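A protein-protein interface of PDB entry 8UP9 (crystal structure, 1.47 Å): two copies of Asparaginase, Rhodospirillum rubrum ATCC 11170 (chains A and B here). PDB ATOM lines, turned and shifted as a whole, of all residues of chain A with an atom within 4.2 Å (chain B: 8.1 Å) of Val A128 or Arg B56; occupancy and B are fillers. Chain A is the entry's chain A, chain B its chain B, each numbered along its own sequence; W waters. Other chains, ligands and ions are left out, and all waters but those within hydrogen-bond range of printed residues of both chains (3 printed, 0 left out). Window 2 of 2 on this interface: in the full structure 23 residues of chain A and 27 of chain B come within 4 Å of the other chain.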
ATOM      1  N   THR A  29     -23.808 -17.218  15.552  1.00  0.00           N
ATOM      2  CA  THR A  29     -25.249 -17.567  15.540  1.00  0.00           C
ATOM      3  C   THR A  29     -25.901 -17.326  16.913  1.00  0.00           C
ATOM      4  O   THR A  29     -27.040 -16.834  16.942  1.00  0.00           O
ATOM      5  CB  THR A  29     -25.439 -19.034  15.124  1.00  0.00           C
ATOM      6  OG1 THR A  29     -24.705 -19.249  13.907  1.00  0.00           O
ATOM      7  CG2 THR A  29     -26.907 -19.394  14.977  1.00  0.00           C
ATOM      8  N   ALA A 126     -23.857 -21.516  19.789  1.00  0.00           N
ATOM      9  CA  ALA A 126     -25.171 -22.210  19.617  1.00  0.00           C
ATOM     10  C   ALA A 126     -25.357 -22.488  18.119  1.00  0.00           C
ATOM     11  O   ALA A 126     -24.946 -21.653  17.300  1.00  0.00           O
ATOM     12  CB  ALA A 126     -26.330 -21.373  20.179  1.00  0.00           C
ATOM     13  N   MET A 127     -26.057 -23.554  17.842  1.00  0.00           N
ATOM     14  CA  MET A 127     -26.485 -23.888  16.473  1.00  0.00           C
ATOM     15  C   MET A 127     -27.723 -23.086  16.080  1.00  0.00           C
ATOM     16  O   MET A 127     -28.003 -22.875  14.913  1.00  0.00           O
ATOM     17  CB  MET A 127     -26.730 -25.381  16.358  1.00  0.00           C
ATOM     18  CG  MET A 127     -25.470 -26.152  16.686  1.00  0.00           C
ATOM     19  SD  MET A 127     -24.057 -25.665  15.571  1.00  0.00           S
ATOM     20  CE  MET A 127     -22.702 -26.588  16.269  1.00  0.00           C
ATOM     21  N   VAL A 128     -28.532 -22.694  17.074  1.00  0.00           N
ATOM     22  CA  VAL A 128     -29.774 -21.916  16.892  1.00  0.00           C
ATOM     23  C   VAL A 128     -29.628 -20.623  17.694  1.00  0.00           C
ATOM     24  O   VAL A 128     -29.179 -20.687  18.859  1.00  0.00           O
ATOM     25  CB  VAL A 128     -30.990 -22.699  17.411  1.00  0.00           C
ATOM     26  CG1 VAL A 128     -32.247 -21.859  17.352  1.00  0.00           C
ATOM     27  CG2 VAL A 128     -31.194 -23.998  16.628  1.00  0.00           C
ATOM     28  N   PRO A 129     -29.885 -19.434  17.103  1.00  0.00           N
ATOM     29  CA  PRO A 129     -29.750 -18.207  17.893  1.00  0.00           C
ATOM     30  C   PRO A 129     -30.471 -18.293  19.246  1.00  0.00           C
ATOM     31  O   PRO A 129     -31.628 -18.792  19.302  1.00  0.00           O
ATOM     32  CB  PRO A 129     -30.368 -17.117  16.986  1.00  0.00           C
ATOM     33  CG  PRO A 129     -30.164 -17.691  15.577  1.00  0.00           C
ATOM     34  CD  PRO A 129     -30.425 -19.168  15.760  1.00  0.00           C
ATOM     35  N   GLY A 130     -29.860 -17.722  20.305  1.00  0.00           N
ATOM     36  CA  GLY A 130     -30.522 -17.697  21.630  1.00  0.00           C
ATOM     37  C   GLY A 130     -31.896 -17.055  21.595  1.00  0.00           C
ATOM     38  O   GLY A 130     -32.792 -17.431  22.380  1.00  0.00           O
ATOM     39  N   VAL A 132     -34.079 -17.150  19.215  1.00  0.00           N
ATOM     40  CA  VAL A 132     -35.051 -17.948  18.463  1.00  0.00           C
ATOM     41  C   VAL A 132     -35.542 -19.087  19.367  1.00  0.00           C
ATOM     42  O   VAL A 132     -34.737 -19.689  20.117  1.00  0.00           O
ATOM     43  CB  VAL A 132     -34.417 -18.504  17.181  1.00  0.00           C
ATOM     44  CG1 VAL A 132     -35.278 -19.585  16.522  1.00  0.00           C
ATOM     45  CG2 VAL A 132     -34.112 -17.378  16.216  1.00  0.00           C
ATOM     46  N   SER A 135     -33.758 -22.810  21.135  1.00  0.00           N
ATOM     47  CA  SER A 135     -32.299 -22.711  21.082  1.00  0.00           C
ATOM     48  C   SER A 135     -31.561 -23.543  22.092  1.00  0.00           C
ATOM     49  O   SER A 135     -32.026 -23.678  23.263  1.00  0.00           O
ATOM     50  CB  SER A 135     -31.839 -21.253  21.209  1.00  0.00           C
ATOM     51  OG  SER A 135     -30.448 -21.164  21.221  1.00  0.00           O
ATOM     52  N   ASP A 136     -30.457 -24.126  21.711  1.00  0.00           N
ATOM     53  CA  ASP A 136     -29.446 -24.816  22.555  1.00  0.00           C
ATOM     54  C   ASP A 136     -28.658 -23.851  23.427  1.00  0.00           C
ATOM     55  O   ASP A 136     -27.864 -24.320  24.261  1.00  0.00           O
ATOM     56  CB  ASP A 136     -28.537 -25.629  21.624  1.00  0.00           C
ATOM     57  CG  ASP A 136     -27.928 -24.882  20.431  1.00  0.00           C
ATOM     58  OD1 ASP A 136     -28.639 -24.071  19.822  1.00  0.00           O
ATOM     59  OD2 ASP A 136     -26.778 -25.217  20.112  1.00  0.00           O
ATOM     60  N   HIS A 160     -22.980 -29.776  22.395  1.00  0.00           N
ATOM     61  CA  HIS A 160     -23.687 -31.067  22.388  1.00  0.00           C
ATOM     62  C   HIS A 160     -23.422 -31.796  23.679  1.00  0.00           C
ATOM     63  O   HIS A 160     -23.537 -33.022  23.741  1.00  0.00           O
ATOM     64  CB  HIS A 160     -23.220 -31.940  21.235  1.00  0.00           C
ATOM     65  CG  HIS A 160     -23.094 -31.236  19.929  1.00  0.00           C
ATOM     66  ND1 HIS A 160     -24.174 -30.612  19.358  1.00  0.00           N
ATOM     67  CD2 HIS A 160     -22.027 -31.028  19.095  1.00  0.00           C
ATOM     68  CE1 HIS A 160     -23.802 -30.106  18.169  1.00  0.00           C
ATOM     69  NE2 HIS A 160     -22.503 -30.324  18.025  1.00  0.00           N
ATOM     70  N   VAL B  51     -35.337 -29.125  28.418  1.00  0.00           N
ATOM     71  CA  VAL B  51     -34.013 -28.523  28.198  1.00  0.00           C
ATOM     72  C   VAL B  51     -33.204 -29.466  27.310  1.00  0.00           C
ATOM     73  O   VAL B  51     -32.527 -28.997  26.386  1.00  0.00           O
ATOM     74  CB  VAL B  51     -33.276 -28.159  29.466  1.00  0.00           C
ATOM     75  CG1 VAL B  51     -31.908 -27.605  29.196  1.00  0.00           C
ATOM     76  CG2 VAL B  51     -34.124 -27.199  30.312  1.00  0.00           C
ATOM     77  N   LEU B  52     -33.156 -30.750  27.630  1.00  0.00           N
ATOM     78  CA  LEU B  52     -32.244 -31.646  26.884  1.00  0.00           C
ATOM     79  C   LEU B  52     -32.772 -31.916  25.477  1.00  0.00           C
ATOM     80  O   LEU B  52     -31.898 -32.134  24.625  1.00  0.00           O
ATOM     81  CB  LEU B  52     -32.043 -32.914  27.684  1.00  0.00           C
ATOM     82  CG  LEU B  52     -31.319 -32.703  28.983  1.00  0.00           C
ATOM     83  CD1 LEU B  52     -30.982 -34.047  29.608  1.00  0.00           C
ATOM     84  CD2 LEU B  52     -30.070 -31.820  28.843  1.00  0.00           C
ATOM     85  N   LYS B  53     -34.059 -31.733  25.222  1.00  0.00           N
ATOM     86  CA  LYS B  53     -34.673 -31.926  23.894  1.00  0.00           C
ATOM     87  C   LYS B  53     -34.015 -30.998  22.908  1.00  0.00           C
ATOM     88  O   LYS B  53     -33.846 -31.407  21.709  1.00  0.00           O
ATOM     89  CB  LYS B  53     -36.174 -31.631  23.832  1.00  0.00           C
ATOM     90  CG  LYS B  53     -36.651 -31.608  22.396  1.00  0.00           C
ATOM     91  CD  LYS B  53     -38.122 -31.584  22.176  1.00  0.00           C
ATOM     92  CE  LYS B  53     -38.423 -31.245  20.733  1.00  0.00           C
ATOM     93  NZ  LYS B  53     -39.876 -31.284  20.487  1.00  0.00           N
ATOM     94  N   THR B  54     -33.645 -29.805  23.315  1.00  0.00           N
ATOM     95  CA  THR B  54     -33.128 -28.792  22.372  1.00  0.00           C
ATOM     96  C   THR B  54     -31.606 -28.663  22.528  1.00  0.00           C
ATOM     97  O   THR B  54     -30.986 -27.824  21.876  1.00  0.00           O
ATOM     98  CB  THR B  54     -33.919 -27.495  22.525  1.00  0.00           C
ATOM     99  OG1 THR B  54     -33.763 -27.014  23.869  1.00  0.00           O
ATOM    100  CG2 THR B  54     -35.368 -27.638  22.063  1.00  0.00           C
ATOM    101  N   ALA B  55     -30.980 -29.437  23.417  1.00  0.00           N
ATOM    102  CA  ALA B  55     -29.533 -29.337  23.689  1.00  0.00           C
ATOM    103  C   ALA B  55     -28.730 -30.056  22.610  1.00  0.00           C
ATOM    104  O   ALA B  55     -27.502 -29.989  22.657  1.00  0.00           O
ATOM    105  CB  ALA B  55     -29.199 -29.940  25.019  1.00  0.00           C
ATOM    106  N   ARG B  56     -29.364 -30.798  21.684  1.00  0.00           N
ATOM    107  CA  ARG B  56     -28.650 -31.375  20.509  1.00  0.00           C
ATOM    108  C   ARG B  56     -27.492 -32.236  21.049  1.00  0.00           C
ATOM    109  O   ARG B  56     -26.344 -32.086  20.578  1.00  0.00           O
ATOM    110  CB  ARG B  56     -28.240 -30.222  19.580  1.00  0.00           C
ATOM    111  CG  ARG B  56     -29.440 -29.523  18.951  1.00  0.00           C
ATOM    112  CD  ARG B  56     -29.079 -28.261  18.172  1.00  0.00           C
ATOM    113  NE  ARG B  56     -30.265 -27.669  17.596  1.00  0.00           N
ATOM    114  CZ  ARG B  56     -30.759 -27.988  16.411  1.00  0.00           C
ATOM    115  NH1 ARG B  56     -30.175 -28.939  15.682  1.00  0.00           N
ATOM    116  NH2 ARG B  56     -31.861 -27.381  15.979  1.00  0.00           N
ATOM    117  N   LEU B  57     -27.767 -33.140  22.021  1.00  0.00           N
ATOM    118  CA  LEU B  57     -26.681 -33.855  22.701  1.00  0.00           C
ATOM    119  C   LEU B  57     -25.998 -34.897  21.794  1.00  0.00           C
ATOM    120  O   LEU B  57     -26.692 -35.576  20.999  1.00  0.00           O
ATOM    121  CB  LEU B  57     -27.246 -34.558  23.938  1.00  0.00           C
ATOM    122  CG  LEU B  57     -27.850 -33.652  25.011  1.00  0.00           C
ATOM    123  CD1 LEU B  57     -28.416 -34.492  26.112  1.00  0.00           C
ATOM    124  CD2 LEU B  57     -26.826 -32.659  25.541  1.00  0.00           C
ATOM    125  N   ALA B  58     -24.709 -35.115  22.013  1.00  0.00           N
ATOM    126  CA  ALA B  58     -23.930 -36.175  21.344  1.00  0.00           C
ATOM    127  C   ALA B  58     -23.923 -37.475  22.152  1.00  0.00           C
ATOM    128  O   ALA B  58     -23.759 -38.552  21.532  1.00  0.00           O
ATOM    129  CB  ALA B  58     -22.518 -35.690  21.170  1.00  0.00           C
ATOM    130  N   GLY B  59     -24.025 -37.378  23.474  1.00  0.00           N
ATOM    131  CA  GLY B  59     -23.757 -38.526  24.344  1.00  0.00           C
ATOM    132  C   GLY B  59     -25.039 -39.223  24.730  1.00  0.00           C
ATOM    133  O   GLY B  59     -26.163 -38.723  24.400  1.00  0.00           O
HETATM  134  O   HOH W   1     -25.423 -28.354  22.149  1.00  0.00           O
HETATM  135  O   HOH W   2     -23.955 -35.284  25.300  1.00  0.00           O
HETATM  136  O   HOH W   3     -31.689 -26.462  19.579  1.00  0.00           O
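Of the 9 printed residues of chain B, 5 touch a printed residue of chain A. Hydrophobic or aromatic side chains of chain B within 4 Å of the printed part of chain A: Leu B57 and Ala B58. Along chain B the printed residues that touch a printed residue of chain A span positions 54 to 58. Of the 10 printed residues of chain A, 4 touch a printed residue of chain B. Hydrophobic or aromatic side chains of chain A that line the printed part of chain B: Val A128 and His A160. Along chain A the printed residues that touch a printed residue of chain B span positions 128 to 160. Among the printed residues, no Asp or Glu carboxylate lies within 4 Å of a Lys or Arg side-chain nitrogen of the other chain.
Among the printed residues, merely in contact across the chains: Val A128 with Arg B56 (3.5 Å), Ser A135 with Thr B54 (3.8 Å), Asp A136 with Thr B54 (3.3 Å), His A160 with Ala B55 (3.97 Å) and His A160 with Leu B57 (3.4 Å).
Val A128 touches just one residue of chain B: Arg B56 (3.5 Å). Pro A129 touches none of the printed residues of chain B. Of the printed residues of chain B, Asp A136 touches Thr B54 (3.3 Å). Lys B53 touches none of the printed residues of chain A. Of the printed residues of chain A, Thr B54 touches Ser A135 (3.8 Å) and Asp A136 (3.3 Å). Arg B56 touches just these residues of chain A: Val A128 and His A160. The nearest printed residue of chain B that does not touch His A160 is Gly B59 (4.4 Å).
A ring nitrogen (ND1) of His A160 is in hydrogen-bond range of the backbone carbonyl oxygen of Arg B56, at 2.9 Å. The backbone NH (N) of Ala B58 sits at hydrogen-bond distance from the backbone carbonyl oxygen (O) of His A160 (3.0 Å).
O of Pro A129 lies close to OG of Ser A135 (3.3 Å). O of Val B51 lies within hydrogen-bond range of OG1 of Thr B54, 3.4 Å away. OD1 of Asp A136 sits at hydrogen-bond distance from N of Val A128, at 3.1 Å. N of Met A127 is in hydrogen-bond range of OD2 of Asp A136. The backbone carbonyl oxygen (O) of Val A128 lies within hydrogen-bond range of the side-chain hydroxyl (OG) of Ser A135, at 2.7 Å.
No position is printed for both chains.
Water W1 lies within hydrogen-bond range of O of Ala B55 (2.7 Å) and N of His A160 (2.8 Å). Water W3 lies within hydrogen-bond range of the guanidinium group of Arg B56 (2.7 Å), the backbone carbonyl oxygen of Thr B54 (2.8 Å) and the backbone NH of Asp A136 (3.4 Å). Water W2 lies within hydrogen-bond range of the backbone NH of Gly B59 (2.8 Å), the backbone carbonyl oxygen of His A160 (2.8 Å) and the backbone NH of Ala B58 (3.4 Å).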
